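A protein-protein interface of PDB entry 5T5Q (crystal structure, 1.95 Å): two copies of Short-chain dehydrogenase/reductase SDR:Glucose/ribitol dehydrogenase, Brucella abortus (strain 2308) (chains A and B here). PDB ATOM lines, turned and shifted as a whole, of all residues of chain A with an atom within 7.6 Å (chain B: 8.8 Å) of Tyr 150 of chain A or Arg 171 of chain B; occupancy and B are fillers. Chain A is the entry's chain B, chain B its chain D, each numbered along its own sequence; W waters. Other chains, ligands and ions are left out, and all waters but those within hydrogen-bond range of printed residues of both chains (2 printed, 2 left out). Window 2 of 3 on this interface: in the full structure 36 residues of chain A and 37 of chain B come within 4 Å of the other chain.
The backbone NH (N) of Phe 101 of chain A sits at hydrogen-bond distance from the side-chain carboxylate (OE2) of Glu 172 of chain B, at 2.7 Å.
The guanidinium group (NH2) of Arg 171 of chain B lies within hydrogen-bond range of the backbone carbonyl oxygen (O) of Arg 147 of chain A (2.9 Å).
NE of Arg 171 of chain B is in hydrogen-bond range of O of Gly 148 of chain A (3.2 Å).
N of Lys 99 of chain A sits at hydrogen-bond distance from O of Val 151 of chain A (2.7 Å).
N of Ala 149 of chain A sits at hydrogen-bond distance from O of Ala 144 of chain A (3.5 Å).
Pro 100 of chain A touches Glu 172 of chain B.
Phe 101 of chain A touches Leu 169 of chain B.
Tyr 146 of chain A touches Arg 167 of chain B (O to CD, 3.5 Å).
CB of Arg 167 of chain B touches CA of Gly 148 of chain A, at 3.6 Å.
Ala 168 of chain B touches Gly 148 of chain A.
O of Ala 149 of chain A touches CA of Ala 168 of chain B (3.5 Å).
Arg 171 of chain B touches Tyr 150 of chain A.
Glu 172 of chain B touches Tyr 150 of chain A.
OE1 of Glu 172 of chain B touches CA of Val 151 of chain A, 3.9 Å away.
Ala 153 of chain A touches Ala 168 of chain B.
Tyr 150 of chain A touches just these residues of chain B: Arg 171 and Glu 172.
Arg 171 of chain B touches just these residues of chain A: Arg 147 (2.9 Å), Gly 148 (3.2 Å), Ala 149 (3.9 Å) and Tyr 150 (3.7 Å).
Gly 148 of chain A touches three residues of chain B.
Val 151 of chain A touches just one residue of chain B: Glu 172 (3.9 Å).
No residue of chain A comes within 4 Å of Ser 170 of chain B.
Of the printed residues of chain B, Tyr 146 of chain A touches Arg 167.
Printed residues of chain B within 4 Å of Arg 147 of chain A: Arg 171.
Printed residues of chain A within 4 Å of Ala 168 of chain B: Gly 148, Ala 149 and Ala 153.
Printed residues of chain A within 4 Å of Leu 169 of chain B: Phe 101 (3.5 Å).
Printed residues of chain A within 4 Å of Glu 172 of chain B: Pro 100, Phe 101, Tyr 150 and Val 151.
Gly 235 of chain B touches none of the printed residues of chain A.
Val 179 of chain B touches none of the printed residues of chain A.
The nearest residue of chain B that does not touch Tyr 150 of chain A is Ala 168 of chain B (5.2 Å).
The nearest printed residue of chain A that does not touch Ala 168 of chain B is Asn 152 of chain A (4.8 Å).
Of the 19 printed residues of chain B, 5 touch a printed residue of chain A.
Printed residues of chain B that touch a printed residue of chain A: Arg 167, Ala 168, Leu 169, Arg 171 and Glu 172.
Hydrophobic or aromatic side chains of chain B within 4 Å of the printed part of chain A: Ala 168 and Leu 169.
Of the 17 printed residues of chain A, 9 touch a printed residue of chain B.
Hydrophobic or aromatic side chains of chain A within 4 Å of the printed part of chain B: Phe 101 and Tyr 150.
Along chain A the printed residues that touch a printed residue of chain B span positions 100 to 153.
Among the printed residues, 14 pairs touch across the chains.
No position is printed for both chains.
Of the 14 pairs that touch across the chains among the printed residues, none has its exchanged pair printed and touching as well.
Water W2 lies within hydrogen-bond range of the backbone carbonyl oxygen of Ala 144 of chain A (2.7 Å), the backbone NH of Ala 149 of chain A (2.8 Å) and the backbone carbonyl oxygen of Ser 164 of chain B (3.1 Å).
Water W1 bridges OE2 of Glu 172 of chain B and N of Phe 101 of chain A.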
ATOM      1  N   TYR A  96     -12.125  18.812 -32.061  1.00  0.00           N
ATOM      2  CA  TYR A  96     -12.106  18.773 -30.602  1.00  0.00           C
ATOM      3  C   TYR A  96     -10.928  19.646 -30.190  1.00  0.00           C
ATOM      4  O   TYR A  96      -9.773  19.225 -30.278  1.00  0.00           O
ATOM      5  CB  TYR A  96     -11.962  17.352 -30.085  1.00  0.00           C
ATOM      6  CG  TYR A  96     -11.863  17.255 -28.581  1.00  0.00           C
ATOM      7  CD1 TYR A  96     -10.637  17.119 -27.946  1.00  0.00           C
ATOM      8  CD2 TYR A  96     -13.002  17.287 -27.804  1.00  0.00           C
ATOM      9  CE1 TYR A  96     -10.553  17.027 -26.564  1.00  0.00           C
ATOM     10  CE2 TYR A  96     -12.933  17.194 -26.420  1.00  0.00           C
ATOM     11  CZ  TYR A  96     -11.709  17.065 -25.810  1.00  0.00           C
ATOM     12  OH  TYR A  96     -11.645  16.970 -24.442  1.00  0.00           O
ATOM     13  N   LYS A  99      -9.690  24.312 -25.062  1.00  0.00           N
ATOM     14  CA  LYS A  99      -9.719  25.769 -24.963  1.00  0.00           C
ATOM     15  C   LYS A  99     -10.424  26.184 -23.681  1.00  0.00           C
ATOM     16  O   LYS A  99     -11.664  26.278 -23.645  1.00  0.00           O
ATOM     17  CB  LYS A  99     -10.409  26.394 -26.168  1.00  0.00           C
ATOM     18  CG  LYS A  99     -10.392  27.912 -26.157  1.00  0.00           C
ATOM     19  CD  LYS A  99      -8.946  28.434 -26.137  1.00  0.00           C
ATOM     20  CE  LYS A  99      -8.186  28.033 -27.414  1.00  0.00           C
ATOM     21  NZ  LYS A  99      -6.837  28.666 -27.543  1.00  0.00           N
ATOM     22  N   PRO A 100      -9.671  26.475 -22.615  1.00  0.00           N
ATOM     23  CA  PRO A 100     -10.288  27.021 -21.396  1.00  0.00           C
ATOM     24  C   PRO A 100     -11.205  28.194 -21.727  1.00  0.00           C
ATOM     25  O   PRO A 100     -10.881  29.041 -22.567  1.00  0.00           O
ATOM     26  CB  PRO A 100      -9.083  27.467 -20.560  1.00  0.00           C
ATOM     27  CG  PRO A 100      -7.959  26.577 -21.013  1.00  0.00           C
ATOM     28  CD  PRO A 100      -8.209  26.324 -22.488  1.00  0.00           C
ATOM     29  N   PHE A 101     -12.368  28.220 -21.058  1.00  0.00           N
ATOM     30  CA  PHE A 101     -13.434  29.151 -21.425  1.00  0.00           C
ATOM     31  C   PHE A 101     -13.003  30.606 -21.307  1.00  0.00           C
ATOM     32  O   PHE A 101     -13.450  31.456 -22.087  1.00  0.00           O
ATOM     33  CB  PHE A 101     -14.682  28.906 -20.573  1.00  0.00           C
ATOM     34  CG  PHE A 101     -15.887  29.654 -21.067  1.00  0.00           C
ATOM     35  CD1 PHE A 101     -16.467  29.320 -22.279  1.00  0.00           C
ATOM     36  CD2 PHE A 101     -16.421  30.708 -20.339  1.00  0.00           C
ATOM     37  CE1 PHE A 101     -17.563  30.008 -22.760  1.00  0.00           C
ATOM     38  CE2 PHE A 101     -17.525  31.400 -20.808  1.00  0.00           C
ATOM     39  CZ  PHE A 101     -18.093  31.052 -22.028  1.00  0.00           C
ATOM     40  N   LEU A 143     -19.022  11.625 -24.853  1.00  0.00           N
ATOM     41  CA  LEU A 143     -19.009  11.629 -23.401  1.00  0.00           C
ATOM     42  C   LEU A 143     -19.095  13.049 -22.851  1.00  0.00           C
ATOM     43  O   LEU A 143     -19.792  13.303 -21.861  1.00  0.00           O
ATOM     44  CB  LEU A 143     -17.741  10.925 -22.923  1.00  0.00           C
ATOM     45  CG  LEU A 143     -17.427  11.054 -21.441  1.00  0.00           C
ATOM     46  CD1 LEU A 143     -18.569  10.451 -20.650  1.00  0.00           C
ATOM     47  CD2 LEU A 143     -16.091  10.388 -21.138  1.00  0.00           C
ATOM     48  N   ALA A 144     -18.415  13.999 -23.498  1.00  0.00           N
ATOM     49  CA  ALA A 144     -18.424  15.374 -23.003  1.00  0.00           C
ATOM     50  C   ALA A 144     -19.840  15.952 -22.925  1.00  0.00           C
ATOM     51  O   ALA A 144     -20.096  16.858 -22.119  1.00  0.00           O
ATOM     52  CB  ALA A 144     -17.542  16.257 -23.891  1.00  0.00           C
ATOM     53  N   TYR A 146     -22.452  14.543 -21.877  1.00  0.00           N
ATOM     54  CA  TYR A 146     -23.116  14.024 -20.702  1.00  0.00           C
ATOM     55  C   TYR A 146     -22.357  14.347 -19.431  1.00  0.00           C
ATOM     56  O   TYR A 146     -22.957  14.793 -18.450  1.00  0.00           O
ATOM     57  CB  TYR A 146     -23.285  12.520 -20.862  1.00  0.00           C
ATOM     58  CG  TYR A 146     -24.211  12.161 -22.004  1.00  0.00           C
ATOM     59  CD1 TYR A 146     -25.580  11.954 -21.776  1.00  0.00           C
ATOM     60  CD2 TYR A 146     -23.733  12.042 -23.312  1.00  0.00           C
ATOM     61  CE1 TYR A 146     -26.424  11.608 -22.822  1.00  0.00           C
ATOM     62  CE2 TYR A 146     -24.581  11.709 -24.366  1.00  0.00           C
ATOM     63  CZ  TYR A 146     -25.923  11.491 -24.119  1.00  0.00           C
ATOM     64  OH  TYR A 146     -26.774  11.130 -25.162  1.00  0.00           O
ATOM     65  N   ARG A 147     -21.039  14.149 -19.446  1.00  0.00           N
ATOM     66  CA  ARG A 147     -20.219  14.372 -18.263  1.00  0.00           C
ATOM     67  C   ARG A 147     -19.930  15.852 -18.034  1.00  0.00           C
ATOM     68  O   ARG A 147     -19.650  16.248 -16.896  1.00  0.00           O
ATOM     69  CB  ARG A 147     -18.914  13.572 -18.391  1.00  0.00           C
ATOM     70  CG  ARG A 147     -17.988  13.636 -17.213  1.00  0.00           C
ATOM     71  CD  ARG A 147     -16.868  12.630 -17.344  1.00  0.00           C
ATOM     72  NE  ARG A 147     -15.919  12.980 -18.398  1.00  0.00           N
ATOM     73  CZ  ARG A 147     -14.759  12.351 -18.578  1.00  0.00           C
ATOM     74  NH1 ARG A 147     -14.430  11.344 -17.770  1.00  0.00           N
ATOM     75  NH2 ARG A 147     -13.933  12.720 -19.550  1.00  0.00           N
ATOM     76  N   GLY A 148     -20.031  16.676 -19.082  1.00  0.00           N
ATOM     77  CA  GLY A 148     -19.631  18.071 -19.028  1.00  0.00           C
ATOM     78  C   GLY A 148     -18.169  18.229 -19.403  1.00  0.00           C
ATOM     79  O   GLY A 148     -17.299  17.696 -18.710  1.00  0.00           O
ATOM     80  N   ALA A 149     -17.871  18.945 -20.487  1.00  0.00           N
ATOM     81  CA  ALA A 149     -16.481  19.083 -20.914  1.00  0.00           C
ATOM     82  C   ALA A 149     -15.657  19.812 -19.866  1.00  0.00           C
ATOM     83  O   ALA A 149     -16.154  20.686 -19.152  1.00  0.00           O
ATOM     84  CB  ALA A 149     -16.385  19.829 -22.253  1.00  0.00           C
ATOM     85  N   TYR A 150     -14.375  19.442 -19.768  1.00  0.00           N
ATOM     86  CA  TYR A 150     -13.515  20.083 -18.780  1.00  0.00           C
ATOM     87  C   TYR A 150     -12.934  21.397 -19.302  1.00  0.00           C
ATOM     88  O   TYR A 150     -12.828  22.368 -18.543  1.00  0.00           O
ATOM     89  CB  TYR A 150     -12.389  19.140 -18.356  1.00  0.00           C
ATOM     90  CG  TYR A 150     -12.846  17.920 -17.580  1.00  0.00           C
ATOM     91  CD1 TYR A 150     -13.151  17.998 -16.216  1.00  0.00           C
ATOM     92  CD2 TYR A 150     -12.961  16.687 -18.208  1.00  0.00           C
ATOM     93  CE1 TYR A 150     -13.564  16.873 -15.511  1.00  0.00           C
ATOM     94  CE2 TYR A 150     -13.375  15.567 -17.516  1.00  0.00           C
ATOM     95  CZ  TYR A 150     -13.675  15.661 -16.176  1.00  0.00           C
ATOM     96  OH  TYR A 150     -14.072  14.529 -15.515  1.00  0.00           O
ATOM     97  N   VAL A 151     -12.536  21.451 -20.580  1.00  0.00           N
ATOM     98  CA  VAL A 151     -11.949  22.662 -21.164  1.00  0.00           C
ATOM     99  C   VAL A 151     -12.356  22.781 -22.627  1.00  0.00           C
ATOM    100  O   VAL A 151     -11.510  23.007 -23.503  1.00  0.00           O
ATOM    101  CB  VAL A 151     -10.408  22.684 -21.049  1.00  0.00           C
ATOM    102  CG1 VAL A 151      -9.967  23.086 -19.649  1.00  0.00           C
ATOM    103  CG2 VAL A 151      -9.815  21.335 -21.461  1.00  0.00           C
ATOM    104  N   ASN A 152     -13.638  22.555 -22.912  1.00  0.00           N
ATOM    105  CA  ASN A 152     -14.128  22.537 -24.286  1.00  0.00           C
ATOM    106  C   ASN A 152     -15.626  22.820 -24.273  1.00  0.00           C
ATOM    107  O   ASN A 152     -16.422  21.954 -24.662  1.00  0.00           O
ATOM    108  CB  ASN A 152     -13.852  21.184 -24.966  1.00  0.00           C
ATOM    109  CG  ASN A 152     -12.692  20.418 -24.327  1.00  0.00           C
ATOM    110  OD1 ASN A 152     -12.811  19.900 -23.213  1.00  0.00           O
ATOM    111  ND2 ASN A 152     -11.563  20.359 -25.023  1.00  0.00           N
ATOM    112  N   ALA A 153     -16.025  23.998 -23.778  1.00  0.00           N
ATOM    113  CA  ALA A 153     -17.455  24.295 -23.661  1.00  0.00           C
ATOM    114  C   ALA A 153     -18.136  24.348 -25.021  1.00  0.00           C
ATOM    115  O   ALA A 153     -19.317  24.002 -25.131  1.00  0.00           O
ATOM    116  CB  ALA A 153     -17.688  25.615 -22.933  1.00  0.00           C
ATOM    117  N   ILE A 186     -13.605   7.341 -24.023  1.00  0.00           N
ATOM    118  CA  ILE A 186     -12.187   7.598 -24.272  1.00  0.00           C
ATOM    119  C   ILE A 186     -11.685   6.563 -25.278  1.00  0.00           C
ATOM    120  O   ILE A 186     -11.608   5.368 -24.970  1.00  0.00           O
ATOM    121  CB  ILE A 186     -11.362   7.559 -22.981  1.00  0.00           C
ATOM    122  CG1 ILE A 186     -12.053   8.375 -21.886  1.00  0.00           C
ATOM    123  CG2 ILE A 186      -9.945   8.116 -23.239  1.00  0.00           C
ATOM    124  CD1 ILE A 186     -12.330   9.805 -22.276  1.00  0.00           C
ATOM    125  N   GLN A 206     -10.647   4.472 -13.683  1.00  0.00           N
ATOM    126  CA  GLN A 206     -12.007   4.986 -13.770  1.00  0.00           C
ATOM    127  C   GLN A 206     -12.891   4.187 -14.724  1.00  0.00           C
ATOM    128  O   GLN A 206     -14.117   4.341 -14.685  1.00  0.00           O
ATOM    129  CB  GLN A 206     -11.950   6.440 -14.231  1.00  0.00           C
ATOM    130  CG  GLN A 206     -11.410   7.401 -13.201  1.00  0.00           C
ATOM    131  CD  GLN A 206     -11.271   8.805 -13.759  1.00  0.00           C
ATOM    132  OE1 GLN A 206     -10.170   9.233 -14.113  1.00  0.00           O
ATOM    133  NE2 GLN A 206     -12.387   9.524 -13.856  1.00  0.00           N
ATOM    134  N   TYR A 245     -18.732   6.289 -17.668  1.00  0.00           N
ATOM    135  CA  TYR A 245     -19.787   7.218 -17.288  1.00  0.00           C
ATOM    136  C   TYR A 245     -21.124   6.564 -17.599  1.00  0.00           C
ATOM    137  O   TYR A 245     -21.295   5.971 -18.670  1.00  0.00           O
ATOM    138  CB  TYR A 245     -19.671   8.537 -18.060  1.00  0.00           C
ATOM    139  CG  TYR A 245     -20.340   9.708 -17.388  1.00  0.00           C
ATOM    140  CD1 TYR A 245     -19.715  10.363 -16.347  1.00  0.00           C
ATOM    141  CD2 TYR A 245     -21.586  10.159 -17.793  1.00  0.00           C
ATOM    142  CE1 TYR A 245     -20.305  11.437 -15.714  1.00  0.00           C
ATOM    143  CE2 TYR A 245     -22.191  11.244 -17.168  1.00  0.00           C
ATOM    144  CZ  TYR A 245     -21.543  11.871 -16.135  1.00  0.00           C
ATOM    145  OH  TYR A 245     -22.110  12.947 -15.502  1.00  0.00           O
ATOM    146  N   SER B 164     -25.815  20.778 -22.176  1.00  0.00           N
ATOM    147  CA  SER B 164     -24.418  20.367 -22.104  1.00  0.00           C
ATOM    148  C   SER B 164     -23.498  21.539 -21.831  1.00  0.00           C
ATOM    149  O   SER B 164     -22.473  21.369 -21.166  1.00  0.00           O
ATOM    150  CB  SER B 164     -24.009  19.669 -23.398  1.00  0.00           C
ATOM    151  OG  SER B 164     -24.687  18.431 -23.511  1.00  0.00           O
ATOM    152  N   MET B 165     -23.825  22.720 -22.363  1.00  0.00           N
ATOM    153  CA  MET B 165     -22.996  23.885 -22.097  1.00  0.00           C
ATOM    154  C   MET B 165     -23.041  24.236 -20.619  1.00  0.00           C
ATOM    155  O   MET B 165     -22.027  24.612 -20.032  1.00  0.00           O
ATOM    156  CB  MET B 165     -23.470  25.055 -22.949  1.00  0.00           C
ATOM    157  CG  MET B 165     -22.557  26.253 -22.943  1.00  0.00           C
ATOM    158  SD  MET B 165     -23.254  27.497 -24.020  1.00  0.00           S
ATOM    159  CE  MET B 165     -22.072  28.843 -23.859  1.00  0.00           C
ATOM    160  N   THR B 166     -24.208  24.050 -19.998  1.00  0.00           N
ATOM    161  CA  THR B 166     -24.360  24.259 -18.566  1.00  0.00           C
ATOM    162  C   THR B 166     -23.443  23.332 -17.777  1.00  0.00           C
ATOM    163  O   THR B 166     -22.810  23.756 -16.806  1.00  0.00           O
ATOM    164  CB  THR B 166     -25.830  24.036 -18.207  1.00  0.00           C
ATOM    165  OG1 THR B 166     -26.620  25.017 -18.904  1.00  0.00           O
ATOM    166  CG2 THR B 166     -26.067  24.145 -16.714  1.00  0.00           C
ATOM    167  N   ARG B 167     -23.378  22.058 -18.170  1.00  0.00           N
ATOM    168  CA  ARG B 167     -22.476  21.120 -17.514  1.00  0.00           C
ATOM    169  C   ARG B 167     -21.013  21.526 -17.682  1.00  0.00           C
ATOM    170  O   ARG B 167     -20.244  21.520 -16.714  1.00  0.00           O
ATOM    171  CB  ARG B 167     -22.721  19.724 -18.076  1.00  0.00           C
ATOM    172  CG  ARG B 167     -24.082  19.152 -17.691  1.00  0.00           C
ATOM    173  CD  ARG B 167     -24.390  17.938 -18.531  1.00  0.00           C
ATOM    174  NE  ARG B 167     -25.645  17.309 -18.141  1.00  0.00           N
ATOM    175  CZ  ARG B 167     -26.366  16.514 -18.926  1.00  0.00           C
ATOM    176  NH1 ARG B 167     -25.977  16.244 -20.176  1.00  0.00           N
ATOM    177  NH2 ARG B 167     -27.481  15.988 -18.461  1.00  0.00           N
ATOM    178  N   ALA B 168     -20.623  21.910 -18.904  1.00  0.00           N
ATOM    179  CA  ALA B 168     -19.242  22.311 -19.170  1.00  0.00           C
ATOM    180  C   ALA B 168     -18.849  23.528 -18.347  1.00  0.00           C
ATOM    181  O   ALA B 168     -17.823  23.524 -17.654  1.00  0.00           O
ATOM    182  CB  ALA B 168     -19.065  22.597 -20.664  1.00  0.00           C
ATOM    183  N   LEU B 169     -19.666  24.583 -18.398  1.00  0.00           N
ATOM    184  CA  LEU B 169     -19.320  25.792 -17.663  1.00  0.00           C
ATOM    185  C   LEU B 169     -19.391  25.580 -16.158  1.00  0.00           C
ATOM    186  O   LEU B 169     -18.648  26.220 -15.408  1.00  0.00           O
ATOM    187  CB  LEU B 169     -20.222  26.955 -18.073  1.00  0.00           C
ATOM    188  CG  LEU B 169     -20.007  27.489 -19.485  1.00  0.00           C
ATOM    189  CD1 LEU B 169     -20.906  28.687 -19.760  1.00  0.00           C
ATOM    190  CD2 LEU B 169     -18.543  27.852 -19.663  1.00  0.00           C
ATOM    191  N   SER B 170     -20.279  24.702 -15.699  1.00  0.00           N
ATOM    192  CA  SER B 170     -20.336  24.393 -14.279  1.00  0.00           C
ATOM    193  C   SER B 170     -18.994  23.862 -13.786  1.00  0.00           C
ATOM    194  O   SER B 170     -18.579  24.148 -12.659  1.00  0.00           O
ATOM    195  CB  SER B 170     -21.474  23.392 -14.039  1.00  0.00           C
ATOM    196  OG  SER B 170     -21.161  22.429 -13.061  1.00  0.00           O
ATOM    197  N   ARG B 171     -18.300  23.079 -14.621  1.00  0.00           N
ATOM    198  CA  ARG B 171     -16.980  22.585 -14.242  1.00  0.00           C
ATOM    199  C   ARG B 171     -15.947  23.705 -14.259  1.00  0.00           C
ATOM    200  O   ARG B 171     -15.133  23.824 -13.335  1.00  0.00           O
ATOM    201  CB  ARG B 171     -16.555  21.443 -15.162  1.00  0.00           C
ATOM    202  CG  ARG B 171     -17.390  20.185 -15.011  1.00  0.00           C
ATOM    203  CD  ARG B 171     -16.707  19.027 -15.707  1.00  0.00           C
ATOM    204  NE  ARG B 171     -17.480  17.808 -15.565  1.00  0.00           N
ATOM    205  CZ  ARG B 171     -17.425  17.022 -14.497  1.00  0.00           C
ATOM    206  NH1 ARG B 171     -16.613  17.336 -13.484  1.00  0.00           N
ATOM    207  NH2 ARG B 171     -18.175  15.925 -14.451  1.00  0.00           N
ATOM    208  N   GLU B 172     -15.981  24.554 -15.284  1.00  0.00           N
ATOM    209  CA  GLU B 172     -14.916  25.532 -15.436  1.00  0.00           C
ATOM    210  C   GLU B 172     -15.037  26.696 -14.466  1.00  0.00           C
ATOM    211  O   GLU B 172     -14.015  27.184 -13.984  1.00  0.00           O
ATOM    212  CB  GLU B 172     -14.881  26.059 -16.871  1.00  0.00           C
ATOM    213  CG  GLU B 172     -14.408  25.024 -17.870  1.00  0.00           C
ATOM    214  CD  GLU B 172     -13.970  25.653 -19.190  1.00  0.00           C
ATOM    215  OE1 GLU B 172     -14.634  25.390 -20.214  1.00  0.00           O
ATOM    216  OE2 GLU B 172     -12.953  26.390 -19.200  1.00  0.00           O
ATOM    217  N   LEU B 173     -16.250  27.125 -14.120  1.00  0.00           N
ATOM    218  CA  LEU B 173     -16.386  28.322 -13.300  1.00  0.00           C
ATOM    219  C   LEU B 173     -16.502  28.017 -11.810  1.00  0.00           C
ATOM    220  O   LEU B 173     -16.464  28.948 -10.995  1.00  0.00           O
ATOM    221  CB  LEU B 173     -17.598  29.137 -13.757  1.00  0.00           C
ATOM    222  CG  LEU B 173     -17.622  29.495 -15.247  1.00  0.00           C
ATOM    223  CD1 LEU B 173     -18.731  30.499 -15.547  1.00  0.00           C
ATOM    224  CD2 LEU B 173     -16.268  30.015 -15.723  1.00  0.00           C
ATOM    225  N   ALA B 174     -16.624  26.741 -11.442  1.00  0.00           N
ATOM    226  CA  ALA B 174     -16.558  26.337 -10.047  1.00  0.00           C
ATOM    227  C   ALA B 174     -15.154  26.594  -9.492  1.00  0.00           C
ATOM    228  O   ALA B 174     -14.174  26.608 -10.243  1.00  0.00           O
ATOM    229  CB  ALA B 174     -16.900  24.850  -9.907  1.00  0.00           C
ATOM    230  N   PRO B 175     -15.025  26.798  -8.172  1.00  0.00           N
ATOM    231  CA  PRO B 175     -16.121  26.850  -7.192  1.00  0.00           C
ATOM    232  C   PRO B 175     -16.751  28.233  -7.025  1.00  0.00           C
ATOM    233  O   PRO B 175     -17.717  28.368  -6.282  1.00  0.00           O
ATOM    234  CB  PRO B 175     -15.447  26.400  -5.893  1.00  0.00           C
ATOM    235  CG  PRO B 175     -14.020  26.733  -6.065  1.00  0.00           C
ATOM    236  CD  PRO B 175     -13.700  26.761  -7.527  1.00  0.00           C
ATOM    237  N   LYS B 176     -16.235  29.239  -7.730  1.00  0.00           N
ATOM    238  CA  LYS B 176     -16.745  30.596  -7.551  1.00  0.00           C
ATOM    239  C   LYS B 176     -18.176  30.757  -8.059  1.00  0.00           C
ATOM    240  O   LYS B 176     -18.998  31.391  -7.389  1.00  0.00           O
ATOM    241  CB  LYS B 176     -15.825  31.598  -8.240  1.00  0.00           C
ATOM    242  CG  LYS B 176     -16.264  33.043  -8.050  1.00  0.00           C
ATOM    243  CD  LYS B 176     -15.093  33.996  -8.296  1.00  0.00           C
ATOM    244  CE  LYS B 176     -14.886  34.274  -9.761  1.00  0.00           C
ATOM    245  NZ  LYS B 176     -15.745  35.407 -10.182  1.00  0.00           N
ATOM    246  N   THR B 177     -18.497  30.216  -9.239  1.00  0.00           N
ATOM    247  CA  THR B 177     -19.785  30.450  -9.881  1.00  0.00           C
ATOM    248  C   THR B 177     -20.471  29.113 -10.125  1.00  0.00           C
ATOM    249  O   THR B 177     -19.824  28.171 -10.599  1.00  0.00           O
ATOM    250  CB  THR B 177     -19.611  31.191 -11.218  1.00  0.00           C
ATOM    251  OG1 THR B 177     -18.879  32.403 -11.015  1.00  0.00           O
ATOM    252  CG2 THR B 177     -20.964  31.543 -11.807  1.00  0.00           C
ATOM    253  N   ARG B 178     -21.775  29.026  -9.803  1.00  0.00           N
ATOM    254  CA  ARG B 178     -22.604  27.868 -10.149  1.00  0.00           C
ATOM    255  C   ARG B 178     -23.363  28.114 -11.454  1.00  0.00           C
ATOM    256  O   ARG B 178     -23.838  29.227 -11.715  1.00  0.00           O
ATOM    257  CB  ARG B 178     -23.599  27.535  -9.028  1.00  0.00           C
ATOM    258  CG  ARG B 178     -22.947  27.073  -7.713  1.00  0.00           C
ATOM    259  CD  ARG B 178     -23.965  26.831  -6.592  1.00  0.00           C
ATOM    260  NE  ARG B 178     -24.743  28.033  -6.288  1.00  0.00           N
ATOM    261  CZ  ARG B 178     -25.994  28.233  -6.684  1.00  0.00           C
ATOM    262  NH1 ARG B 178     -26.621  27.293  -7.378  1.00  0.00           N
ATOM    263  NH2 ARG B 178     -26.619  29.359  -6.379  1.00  0.00           N
ATOM    264  N   VAL B 179     -23.473  27.070 -12.279  1.00  0.00           N
ATOM    265  CA  VAL B 179     -24.128  27.164 -13.581  1.00  0.00           C
ATOM    266  C   VAL B 179     -25.188  26.067 -13.668  1.00  0.00           C
ATOM    267  O   VAL B 179     -24.858  24.880 -13.580  1.00  0.00           O
ATOM    268  CB  VAL B 179     -23.129  27.043 -14.746  1.00  0.00           C
ATOM    269  CG1 VAL B 179     -23.831  27.326 -16.059  1.00  0.00           C
ATOM    270  CG2 VAL B 179     -21.940  27.980 -14.546  1.00  0.00           C
ATOM    271  N   THR B 234     -25.008  22.400  -8.922  1.00  0.00           N
ATOM    272  CA  THR B 234     -24.378  23.008 -10.079  1.00  0.00           C
ATOM    273  C   THR B 234     -24.320  22.008 -11.223  1.00  0.00           C
ATOM    274  O   THR B 234     -24.236  20.794 -11.012  1.00  0.00           O
ATOM    275  CB  THR B 234     -22.983  23.559  -9.729  1.00  0.00           C
ATOM    276  OG1 THR B 234     -22.583  24.463 -10.753  1.00  0.00           O
ATOM    277  CG2 THR B 234     -21.963  22.444  -9.612  1.00  0.00           C
ATOM    278  N   GLY B 235     -24.405  22.537 -12.439  1.00  0.00           N
ATOM    279  CA  GLY B 235     -24.417  21.709 -13.626  1.00  0.00           C
ATOM    280  C   GLY B 235     -25.776  21.151 -13.989  1.00  0.00           C
ATOM    281  O   GLY B 235     -25.875  20.414 -14.978  1.00  0.00           O
ATOM    282  N   GLU B 236     -26.816  21.488 -13.226  1.00  0.00           N
ATOM    283  CA  GLU B 236     -28.101  20.794 -13.232  1.00  0.00           C
ATOM    284  C   GLU B 236     -29.163  21.610 -13.972  1.00  0.00           C
ATOM    285  O   GLU B 236     -29.313  22.809 -13.722  1.00  0.00           O
ATOM    286  CB  GLU B 236     -28.520  20.518 -11.774  1.00  0.00           C
ATOM    287  CG  GLU B 236     -29.968  20.038 -11.536  1.00  0.00           C
ATOM    288  CD  GLU B 236     -30.169  18.589 -11.943  1.00  0.00           C
ATOM    289  OE1 GLU B 236     -29.425  18.117 -12.830  1.00  0.00           O
ATOM    290  OE2 GLU B 236     -31.063  17.925 -11.391  1.00  0.00           O
HETATM  291  O   HOH W   1     -11.272  28.853 -17.901  1.00  0.00           O
HETATM  292  O   HOH W   2     -20.147  19.522 -22.025  1.00  0.00           O
